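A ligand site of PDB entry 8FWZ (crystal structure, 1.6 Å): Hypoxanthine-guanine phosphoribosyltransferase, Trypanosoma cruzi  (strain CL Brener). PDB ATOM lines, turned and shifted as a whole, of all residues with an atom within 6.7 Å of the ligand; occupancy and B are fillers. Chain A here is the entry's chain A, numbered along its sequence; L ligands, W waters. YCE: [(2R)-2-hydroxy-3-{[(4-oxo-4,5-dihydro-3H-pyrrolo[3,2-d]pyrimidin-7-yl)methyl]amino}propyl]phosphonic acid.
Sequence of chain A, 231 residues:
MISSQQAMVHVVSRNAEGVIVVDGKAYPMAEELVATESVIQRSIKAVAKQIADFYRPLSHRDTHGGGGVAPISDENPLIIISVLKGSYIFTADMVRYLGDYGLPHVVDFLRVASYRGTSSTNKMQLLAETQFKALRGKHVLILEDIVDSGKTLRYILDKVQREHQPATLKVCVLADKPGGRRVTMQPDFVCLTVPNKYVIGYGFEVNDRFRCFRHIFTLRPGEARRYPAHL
The backbone carbonyl oxygen of Val 199 is in hydrogen-bond range of a nitrogen (N03) of the ligand. The backbone NH (N) of Asp 148 lies within hydrogen-bond range of an oxygen (O17) of the ligand (3.2 Å). O01 of the ligand lies within hydrogen-bond range of N of Val 199 (3.1 Å). O18 of the ligand lies within hydrogen-bond range of OG of Ser 149, 3.1 Å away. A nitrogen (N08) of the ligand lies within hydrogen-bond range of the side-chain carboxylate of Asp 148 (3.0 Å). O18 of the ligand lies within hydrogen-bond range of N of Thr 152 (3.1 Å). The backbone NH (N) of Ser 149 lies within hydrogen-bond range of an oxygen (O19) of the ligand (3.2 Å). The backbone NH of Gly 150 sits at hydrogen-bond distance from an oxygen (O17) of the ligand (3.1 Å). The side-chain amino group (NZ) of Lys 177 is in hydrogen-bond range of an oxygen (O01) of the ligand (3.1 Å). The side-chain hydroxyl (OG1) of Thr 152 lies within hydrogen-bond range of an oxygen (O18) of the ligand, 2.8 Å away.
The backbone carbonyl oxygen (O) of Lys 197 sits at hydrogen-bond distance from the side-chain amino group (NZ) of Lys 177. The side-chain hydroxyl (OG) of Ser 149 is in hydrogen-bond range of the backbone NH (N) of Lys 151, 3.2 Å away. The side-chain hydroxyl of Thr 152 lies close to the side-chain sulfur of Met 124, 3.8 Å away. The side-chain carboxylate (OD2) of Asp 148 lies within salt-bridge range of the side-chain amino group (NZ) of Lys 177, at 2.9 Å. The backbone NH (N) of Lys 177 sits at hydrogen-bond distance from the backbone carbonyl oxygen (O) of Val 147, at 3.1 Å. The backbone carbonyl oxygen (O) of Glu 205 lies within hydrogen-bond range of the side-chain hydroxyl (OH) of Tyr 198, 2.7 Å away.
Ile 146 touches the ligand. N of Lys 151 touches O18 of the ligand (3.7 Å). CZ of Tyr 198 touches C04 of the ligand, at 3.3 Å. O of Glu 205 touches C04 of the ligand, 3.98 Å away. Hydrophobic or aromatic side chains that line the ligand: Ile 146, Tyr 198 and Val 199. The nearest printed residue that does not touch the ligand is Phe 204 (4.03 Å).
Water W3 lies within hydrogen-bond range of an oxygen (O17) of the ligand (2.6 Å) and the backbone NH (N) of Leu 153 (3.0 Å). Water W1 lies within hydrogen-bond range of N05 of the ligand (2.9 Å) and N of Glu 205 (3.1 Å). Water W2 bridges the side-chain carboxylate (OE2) of Glu 205 and a nitrogen (N12) of the ligand.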
ATOM      1  N   VAL A 112      -2.446 -31.719  -1.894  1.00  0.00           N
ATOM      2  CA  VAL A 112      -1.887 -32.612  -0.849  1.00  0.00           C
ATOM      3  C   VAL A 112      -2.995 -32.946   0.148  1.00  0.00           C
ATOM      4  O   VAL A 112      -3.942 -32.176   0.227  1.00  0.00           O
ATOM      5  CB  VAL A 112      -0.687 -31.993  -0.109  1.00  0.00           C
ATOM      6  CG1 VAL A 112       0.605 -32.134  -0.926  1.00  0.00           C
ATOM      7  CG2 VAL A 112      -0.948 -30.528   0.266  1.00  0.00           C
ATOM      8  N   SER A 114      -3.680 -35.316   4.188  1.00  0.00           N
ATOM      9  CA  SER A 114      -3.148 -36.107   5.316  1.00  0.00           C
ATOM     10  C   SER A 114      -4.041 -37.319   5.544  1.00  0.00           C
ATOM     11  O   SER A 114      -5.246 -37.194   5.349  1.00  0.00           O
ATOM     12  CB  SER A 114      -3.053 -35.262   6.573  1.00  0.00           C
ATOM     13  OG  SER A 114      -4.337 -34.730   6.923  1.00  0.00           O
ATOM     14  N   MET A 124       1.389 -37.270   5.336  1.00  0.00           N
ATOM     15  CA  MET A 124       0.990 -36.536   4.106  1.00  0.00           C
ATOM     16  C   MET A 124       1.082 -37.439   2.872  1.00  0.00           C
ATOM     17  O   MET A 124       1.894 -38.344   2.877  1.00  0.00           O
ATOM     18  CB  MET A 124       1.877 -35.297   3.893  1.00  0.00           C
ATOM     19  CG  MET A 124       1.845 -34.277   5.038  1.00  0.00           C
ATOM     20  SD  MET A 124       0.204 -33.603   5.325  1.00  0.00           S
ATOM     21  CE  MET A 124      -0.210 -32.986   3.686  1.00  0.00           C
ATOM     22  N   GLU A 144       0.273 -20.805  -0.605  1.00  0.00           N
ATOM     23  CA  GLU A 144      -0.472 -21.718   0.297  1.00  0.00           C
ATOM     24  C   GLU A 144      -1.468 -20.877   1.104  1.00  0.00           C
ATOM     25  O   GLU A 144      -1.211 -19.715   1.323  1.00  0.00           O
ATOM     26  CB  GLU A 144       0.501 -22.495   1.195  1.00  0.00           C
ATOM     27  CG  GLU A 144      -0.128 -23.385   2.279  1.00  0.00           C
ATOM     28  CD  GLU A 144      -0.941 -24.574   1.783  1.00  0.00           C
ATOM     29  OE1 GLU A 144      -0.665 -25.725   2.185  1.00  0.00           O
ATOM     30  OE2 GLU A 144      -1.874 -24.358   1.023  1.00  0.00           O
ATOM     31  N   ASP A 145      -2.586 -21.477   1.485  1.00  0.00           N
ATOM     32  CA  ASP A 145      -3.655 -20.774   2.235  1.00  0.00           C
ATOM     33  C   ASP A 145      -3.164 -20.483   3.665  1.00  0.00           C
ATOM     34  O   ASP A 145      -3.318 -19.354   4.122  1.00  0.00           O
ATOM     35  CB  ASP A 145      -4.948 -21.610   2.251  1.00  0.00           C
ATOM     36  CG  ASP A 145      -4.841 -23.025   2.789  1.00  0.00           C
ATOM     37  OD1 ASP A 145      -3.745 -23.522   2.939  1.00  0.00           O
ATOM     38  OD2 ASP A 145      -5.873 -23.626   3.028  1.00  0.00           O
ATOM     39  N   ILE A 146      -2.617 -21.471   4.342  1.00  0.00           N
ATOM     40  CA  ILE A 146      -2.269 -21.309   5.777  1.00  0.00           C
ATOM     41  C   ILE A 146      -1.099 -22.194   6.183  1.00  0.00           C
ATOM     42  O   ILE A 146      -0.936 -23.248   5.581  1.00  0.00           O
ATOM     43  CB  ILE A 146      -3.502 -21.595   6.686  1.00  0.00           C
ATOM     44  CG1 ILE A 146      -3.256 -21.192   8.150  1.00  0.00           C
ATOM     45  CG2 ILE A 146      -3.967 -23.047   6.567  1.00  0.00           C
ATOM     46  CD1 ILE A 146      -4.549 -21.037   8.993  1.00  0.00           C
ATOM     47  N   VAL A 147      -0.284 -21.695   7.103  1.00  0.00           N
ATOM     48  CA  VAL A 147       0.762 -22.515   7.763  1.00  0.00           C
ATOM     49  C   VAL A 147       0.228 -22.648   9.191  1.00  0.00           C
ATOM     50  O   VAL A 147      -0.022 -21.617   9.816  1.00  0.00           O
ATOM     51  CB  VAL A 147       2.183 -21.919   7.684  1.00  0.00           C
ATOM     52  CG1 VAL A 147       2.266 -20.491   8.246  1.00  0.00           C
ATOM     53  CG2 VAL A 147       3.200 -22.839   8.361  1.00  0.00           C
ATOM     54  N   ASP A 148      -0.031 -23.860   9.666  1.00  0.00           N
ATOM     55  CA  ASP A 148      -0.586 -24.112  11.019  1.00  0.00           C
ATOM     56  C   ASP A 148       0.450 -24.980  11.752  1.00  0.00           C
ATOM     57  O   ASP A 148       1.341 -24.408  12.377  1.00  0.00           O
ATOM     58  CB  ASP A 148      -2.007 -24.659  10.876  1.00  0.00           C
ATOM     59  CG  ASP A 148      -2.770 -24.839  12.178  1.00  0.00           C
ATOM     60  OD1 ASP A 148      -2.137 -24.900  13.218  1.00  0.00           O
ATOM     61  OD2 ASP A 148      -4.006 -24.914  12.130  1.00  0.00           O
ATOM     62  N   SER A 149       0.398 -26.303  11.614  1.00  0.00           N
ATOM     63  CA  SER A 149       1.416 -27.230  12.189  1.00  0.00           C
ATOM     64  C   SER A 149       2.733 -27.084  11.438  1.00  0.00           C
ATOM     65  O   SER A 149       3.777 -27.286  12.048  1.00  0.00           O
ATOM     66  CB  SER A 149       0.995 -28.689  12.122  1.00  0.00           C
ATOM     67  OG  SER A 149       0.941 -29.127  10.767  1.00  0.00           O
ATOM     68  N   GLY A 150       2.685 -26.813  10.138  1.00  0.00           N
ATOM     69  CA  GLY A 150       3.862 -26.704   9.258  1.00  0.00           C
ATOM     70  C   GLY A 150       4.151 -28.005   8.523  1.00  0.00           C
ATOM     71  O   GLY A 150       5.056 -28.022   7.715  1.00  0.00           O
ATOM     72  N   LYS A 151       3.404 -29.066   8.788  1.00  0.00           N
ATOM     73  CA  LYS A 151       3.707 -30.402   8.219  1.00  0.00           C
ATOM     74  C   LYS A 151       3.436 -30.426   6.709  1.00  0.00           C
ATOM     75  O   LYS A 151       4.206 -31.022   5.990  1.00  0.00           O
ATOM     76  CB  LYS A 151       2.866 -31.491   8.896  1.00  0.00           C
ATOM     77  CG  LYS A 151       3.101 -31.683  10.390  1.00  0.00           C
ATOM     78  CD  LYS A 151       2.041 -32.589  11.064  1.00  0.00           C
ATOM     79  CE  LYS A 151       1.865 -32.352  12.569  1.00  0.00           C
ATOM     80  NZ  LYS A 151       0.422 -32.397  12.988  1.00  0.00           N
ATOM     81  N   THR A 152       2.348 -29.798   6.293  1.00  0.00           N
ATOM     82  CA  THR A 152       1.958 -29.779   4.854  1.00  0.00           C
ATOM     83  C   THR A 152       3.086 -29.126   4.053  1.00  0.00           C
ATOM     84  O   THR A 152       3.514 -29.694   3.045  1.00  0.00           O
ATOM     85  CB  THR A 152       0.580 -29.113   4.648  1.00  0.00           C
ATOM     86  OG1 THR A 152      -0.394 -29.898   5.325  1.00  0.00           O
ATOM     87  CG2 THR A 152       0.248 -28.936   3.175  1.00  0.00           C
ATOM     88  N   LEU A 153       3.562 -27.965   4.470  1.00  0.00           N
ATOM     89  CA  LEU A 153       4.581 -27.200   3.717  1.00  0.00           C
ATOM     90  C   LEU A 153       5.954 -27.893   3.814  1.00  0.00           C
ATOM     91  O   LEU A 153       6.685 -27.854   2.854  1.00  0.00           O
ATOM     92  CB  LEU A 153       4.634 -25.741   4.173  1.00  0.00           C
ATOM     93  CG  LEU A 153       3.603 -24.795   3.553  1.00  0.00           C
ATOM     94  CD1 LEU A 153       3.524 -23.472   4.331  1.00  0.00           C
ATOM     95  CD2 LEU A 153       3.931 -24.527   2.070  1.00  0.00           C
ATOM     96  N   LYS A 177      -0.823 -19.094  11.347  1.00  0.00           N
ATOM     97  CA  LYS A 177      -1.397 -19.377  12.695  1.00  0.00           C
ATOM     98  C   LYS A 177      -0.162 -19.694  13.539  1.00  0.00           C
ATOM     99  O   LYS A 177       0.233 -20.845  13.576  1.00  0.00           O
ATOM    100  CB  LYS A 177      -2.404 -20.539  12.684  1.00  0.00           C
ATOM    101  CG  LYS A 177      -3.130 -20.750  14.005  1.00  0.00           C
ATOM    102  CD  LYS A 177      -4.063 -21.962  14.025  1.00  0.00           C
ATOM    103  CE  LYS A 177      -5.079 -21.970  12.888  1.00  0.00           C
ATOM    104  NZ  LYS A 177      -6.043 -23.113  13.002  1.00  0.00           N
ATOM    105  N   GLY A 180       0.093 -22.782  16.184  1.00  0.00           N
ATOM    106  CA  GLY A 180      -0.154 -24.156  15.721  1.00  0.00           C
ATOM    107  C   GLY A 180       1.127 -24.933  15.406  1.00  0.00           C
ATOM    108  O   GLY A 180       1.028 -26.144  15.299  1.00  0.00           O
ATOM    109  N   VAL A 194      -3.361 -15.005  12.065  1.00  0.00           N
ATOM    110  CA  VAL A 194      -4.696 -15.397  12.564  1.00  0.00           C
ATOM    111  C   VAL A 194      -4.552 -15.914  13.998  1.00  0.00           C
ATOM    112  O   VAL A 194      -3.461 -16.297  14.378  1.00  0.00           O
ATOM    113  CB  VAL A 194      -5.349 -16.462  11.632  1.00  0.00           C
ATOM    114  CG1 VAL A 194      -5.577 -15.870  10.238  1.00  0.00           C
ATOM    115  CG2 VAL A 194      -4.551 -17.762  11.550  1.00  0.00           C
ATOM    116  N   LYS A 197      -6.994 -20.635  16.401  1.00  0.00           N
ATOM    117  CA  LYS A 197      -8.375 -21.140  16.366  1.00  0.00           C
ATOM    118  C   LYS A 197      -8.650 -21.637  14.942  1.00  0.00           C
ATOM    119  O   LYS A 197      -7.950 -21.204  14.050  1.00  0.00           O
ATOM    120  CB  LYS A 197      -9.347 -19.990  16.669  1.00  0.00           C
ATOM    121  CG  LYS A 197      -9.274 -19.386  18.077  1.00  0.00           C
ATOM    122  CD  LYS A 197      -9.713 -20.358  19.200  1.00  0.00           C
ATOM    123  CE  LYS A 197     -10.451 -19.666  20.340  1.00  0.00           C
ATOM    124  NZ  LYS A 197      -9.633 -18.564  20.949  1.00  0.00           N
ATOM    125  N   TYR A 198      -9.676 -22.431  14.750  1.00  0.00           N
ATOM    126  CA  TYR A 198     -10.072 -22.905  13.403  1.00  0.00           C
ATOM    127  C   TYR A 198     -10.668 -21.702  12.660  1.00  0.00           C
ATOM    128  O   TYR A 198     -11.664 -21.176  13.125  1.00  0.00           O
ATOM    129  CB  TYR A 198     -11.057 -24.071  13.468  1.00  0.00           C
ATOM    130  CG  TYR A 198     -11.216 -24.807  12.156  1.00  0.00           C
ATOM    131  CD1 TYR A 198     -12.178 -24.457  11.238  1.00  0.00           C
ATOM    132  CD2 TYR A 198     -10.359 -25.853  11.840  1.00  0.00           C
ATOM    133  CE1 TYR A 198     -12.320 -25.143  10.037  1.00  0.00           C
ATOM    134  CE2 TYR A 198     -10.474 -26.539  10.651  1.00  0.00           C
ATOM    135  CZ  TYR A 198     -11.463 -26.184   9.745  1.00  0.00           C
ATOM    136  OH  TYR A 198     -11.543 -26.892   8.577  1.00  0.00           O
ATOM    137  N   VAL A 199     -10.058 -21.307  11.527  1.00  0.00           N
ATOM    138  CA  VAL A 199     -10.543 -20.158  10.707  1.00  0.00           C
ATOM    139  C   VAL A 199     -11.422 -20.639   9.538  1.00  0.00           C
ATOM    140  O   VAL A 199     -11.271 -21.739   9.087  1.00  0.00           O
ATOM    141  CB  VAL A 199      -9.371 -19.262  10.225  1.00  0.00           C
ATOM    142  CG1 VAL A 199      -8.747 -18.500  11.401  1.00  0.00           C
ATOM    143  CG2 VAL A 199      -8.296 -20.028   9.439  1.00  0.00           C
ATOM    144  N   ILE A 200     -12.344 -19.812   9.091  1.00  0.00           N
ATOM    145  CA  ILE A 200     -13.235 -20.136   7.947  1.00  0.00           C
ATOM    146  C   ILE A 200     -13.360 -18.872   7.103  1.00  0.00           C
ATOM    147  O   ILE A 200     -13.135 -17.810   7.620  1.00  0.00           O
ATOM    148  CB  ILE A 200     -14.614 -20.675   8.399  1.00  0.00           C
ATOM    149  CG1 ILE A 200     -15.327 -19.703   9.354  1.00  0.00           C
ATOM    150  CG2 ILE A 200     -14.486 -22.084   9.015  1.00  0.00           C
ATOM    151  CD1 ILE A 200     -16.846 -19.907   9.428  1.00  0.00           C
ATOM    152  N   GLY A 203     -11.500 -19.051   1.307  1.00  0.00           N
ATOM    153  CA  GLY A 203     -10.760 -20.298   1.010  1.00  0.00           C
ATOM    154  C   GLY A 203     -10.797 -21.313   2.141  1.00  0.00           C
ATOM    155  O   GLY A 203     -10.632 -22.489   1.857  1.00  0.00           O
ATOM    156  N   PHE A 204     -10.991 -20.876   3.387  1.00  0.00           N
ATOM    157  CA  PHE A 204     -10.977 -21.764   4.575  1.00  0.00           C
ATOM    158  C   PHE A 204     -12.360 -22.416   4.691  1.00  0.00           C
ATOM    159  O   PHE A 204     -13.330 -21.764   4.503  1.00  0.00           O
ATOM    160  CB  PHE A 204     -10.488 -21.024   5.832  1.00  0.00           C
ATOM    161  CG  PHE A 204      -9.096 -20.460   5.696  1.00  0.00           C
ATOM    162  CD1 PHE A 204      -8.030 -21.304   5.448  1.00  0.00           C
ATOM    163  CD2 PHE A 204      -8.856 -19.100   5.804  1.00  0.00           C
ATOM    164  CE1 PHE A 204      -6.750 -20.793   5.317  1.00  0.00           C
ATOM    165  CE2 PHE A 204      -7.579 -18.592   5.682  1.00  0.00           C
ATOM    166  CZ  PHE A 204      -6.526 -19.439   5.438  1.00  0.00           C
ATOM    167  N   GLU A 205     -12.409 -23.701   4.991  1.00  0.00           N
ATOM    168  CA  GLU A 205     -13.660 -24.476   4.885  1.00  0.00           C
ATOM    169  C   GLU A 205     -14.035 -25.345   6.086  1.00  0.00           C
ATOM    170  O   GLU A 205     -13.191 -25.509   6.899  1.00  0.00           O
ATOM    171  CB  GLU A 205     -13.449 -25.517   3.779  1.00  0.00           C
ATOM    172  CG  GLU A 205     -12.136 -26.338   3.961  1.00  0.00           C
ATOM    173  CD  GLU A 205     -12.111 -27.837   3.675  1.00  0.00           C
ATOM    174  OE1 GLU A 205     -12.915 -28.310   2.879  1.00  0.00           O
ATOM    175  OE2 GLU A 205     -11.245 -28.537   4.221  1.00  0.00           O
ATOM    176  N   VAL A 206     -15.283 -25.805   6.144  1.00  0.00           N
ATOM    177  CA  VAL A 206     -15.721 -26.892   7.045  1.00  0.00           C
ATOM    178  C   VAL A 206     -16.410 -27.859   6.068  1.00  0.00           C
ATOM    179  O   VAL A 206     -17.505 -27.561   5.697  1.00  0.00           O
ATOM    180  CB  VAL A 206     -16.640 -26.438   8.200  1.00  0.00           C
ATOM    181  CG1 VAL A 206     -17.312 -27.637   8.890  1.00  0.00           C
ATOM    182  CG2 VAL A 206     -15.890 -25.575   9.211  1.00  0.00           C
HETATM  183  C10 YCE L   1      -6.188 -26.466   8.064  1.00  0.00           C
HETATM  184  N12 YCE L   1      -5.485 -27.082   5.770  1.00  0.00           N
HETATM  185  C13 YCE L   1      -4.151 -26.503   5.962  1.00  0.00           C
HETATM  186  C15 YCE L   1      -1.762 -26.873   6.795  1.00  0.00           C
HETATM  187  C02 YCE L   1      -7.979 -23.757   9.556  1.00  0.00           C
HETATM  188  C04 YCE L   1      -9.465 -24.409   7.758  1.00  0.00           C
HETATM  189  C06 YCE L   1      -7.252 -25.608   8.159  1.00  0.00           C
HETATM  190  C07 YCE L   1      -6.970 -24.804   9.217  1.00  0.00           C
HETATM  191  C09 YCE L   1      -5.299 -26.116   9.090  1.00  0.00           C
HETATM  192  C11 YCE L   1      -6.103 -27.570   6.998  1.00  0.00           C
HETATM  193  C14 YCE L   1      -3.174 -27.442   6.706  1.00  0.00           C
HETATM  194  N03 YCE L   1      -9.181 -23.573   8.860  1.00  0.00           N
HETATM  195  N05 YCE L   1      -8.504 -25.437   7.404  1.00  0.00           N
HETATM  196  N08 YCE L   1      -5.806 -25.110   9.752  1.00  0.00           N
HETATM  197  O01 YCE L   1      -7.733 -23.100  10.424  1.00  0.00           O
HETATM  198  O17 YCE L   1       0.324 -26.619   8.156  1.00  0.00           O
HETATM  199  O18 YCE L   1      -0.195 -28.916   7.924  1.00  0.00           O
HETATM  200  O19 YCE L   1      -1.468 -27.706   9.449  1.00  0.00           O
HETATM  201  O20 YCE L   1      -3.195 -28.732   6.152  1.00  0.00           O
HETATM  202  P16 YCE L   1      -0.740 -27.576   8.174  1.00  0.00           P
HETATM  203  O   HOH W   1      -9.641 -25.069   4.783  1.00  0.00           O
HETATM  204  O   HOH W   2      -8.198 -28.579   4.431  1.00  0.00           O
HETATM  205  O   HOH W   3       2.240 -26.133   6.420  1.00  0.00           O
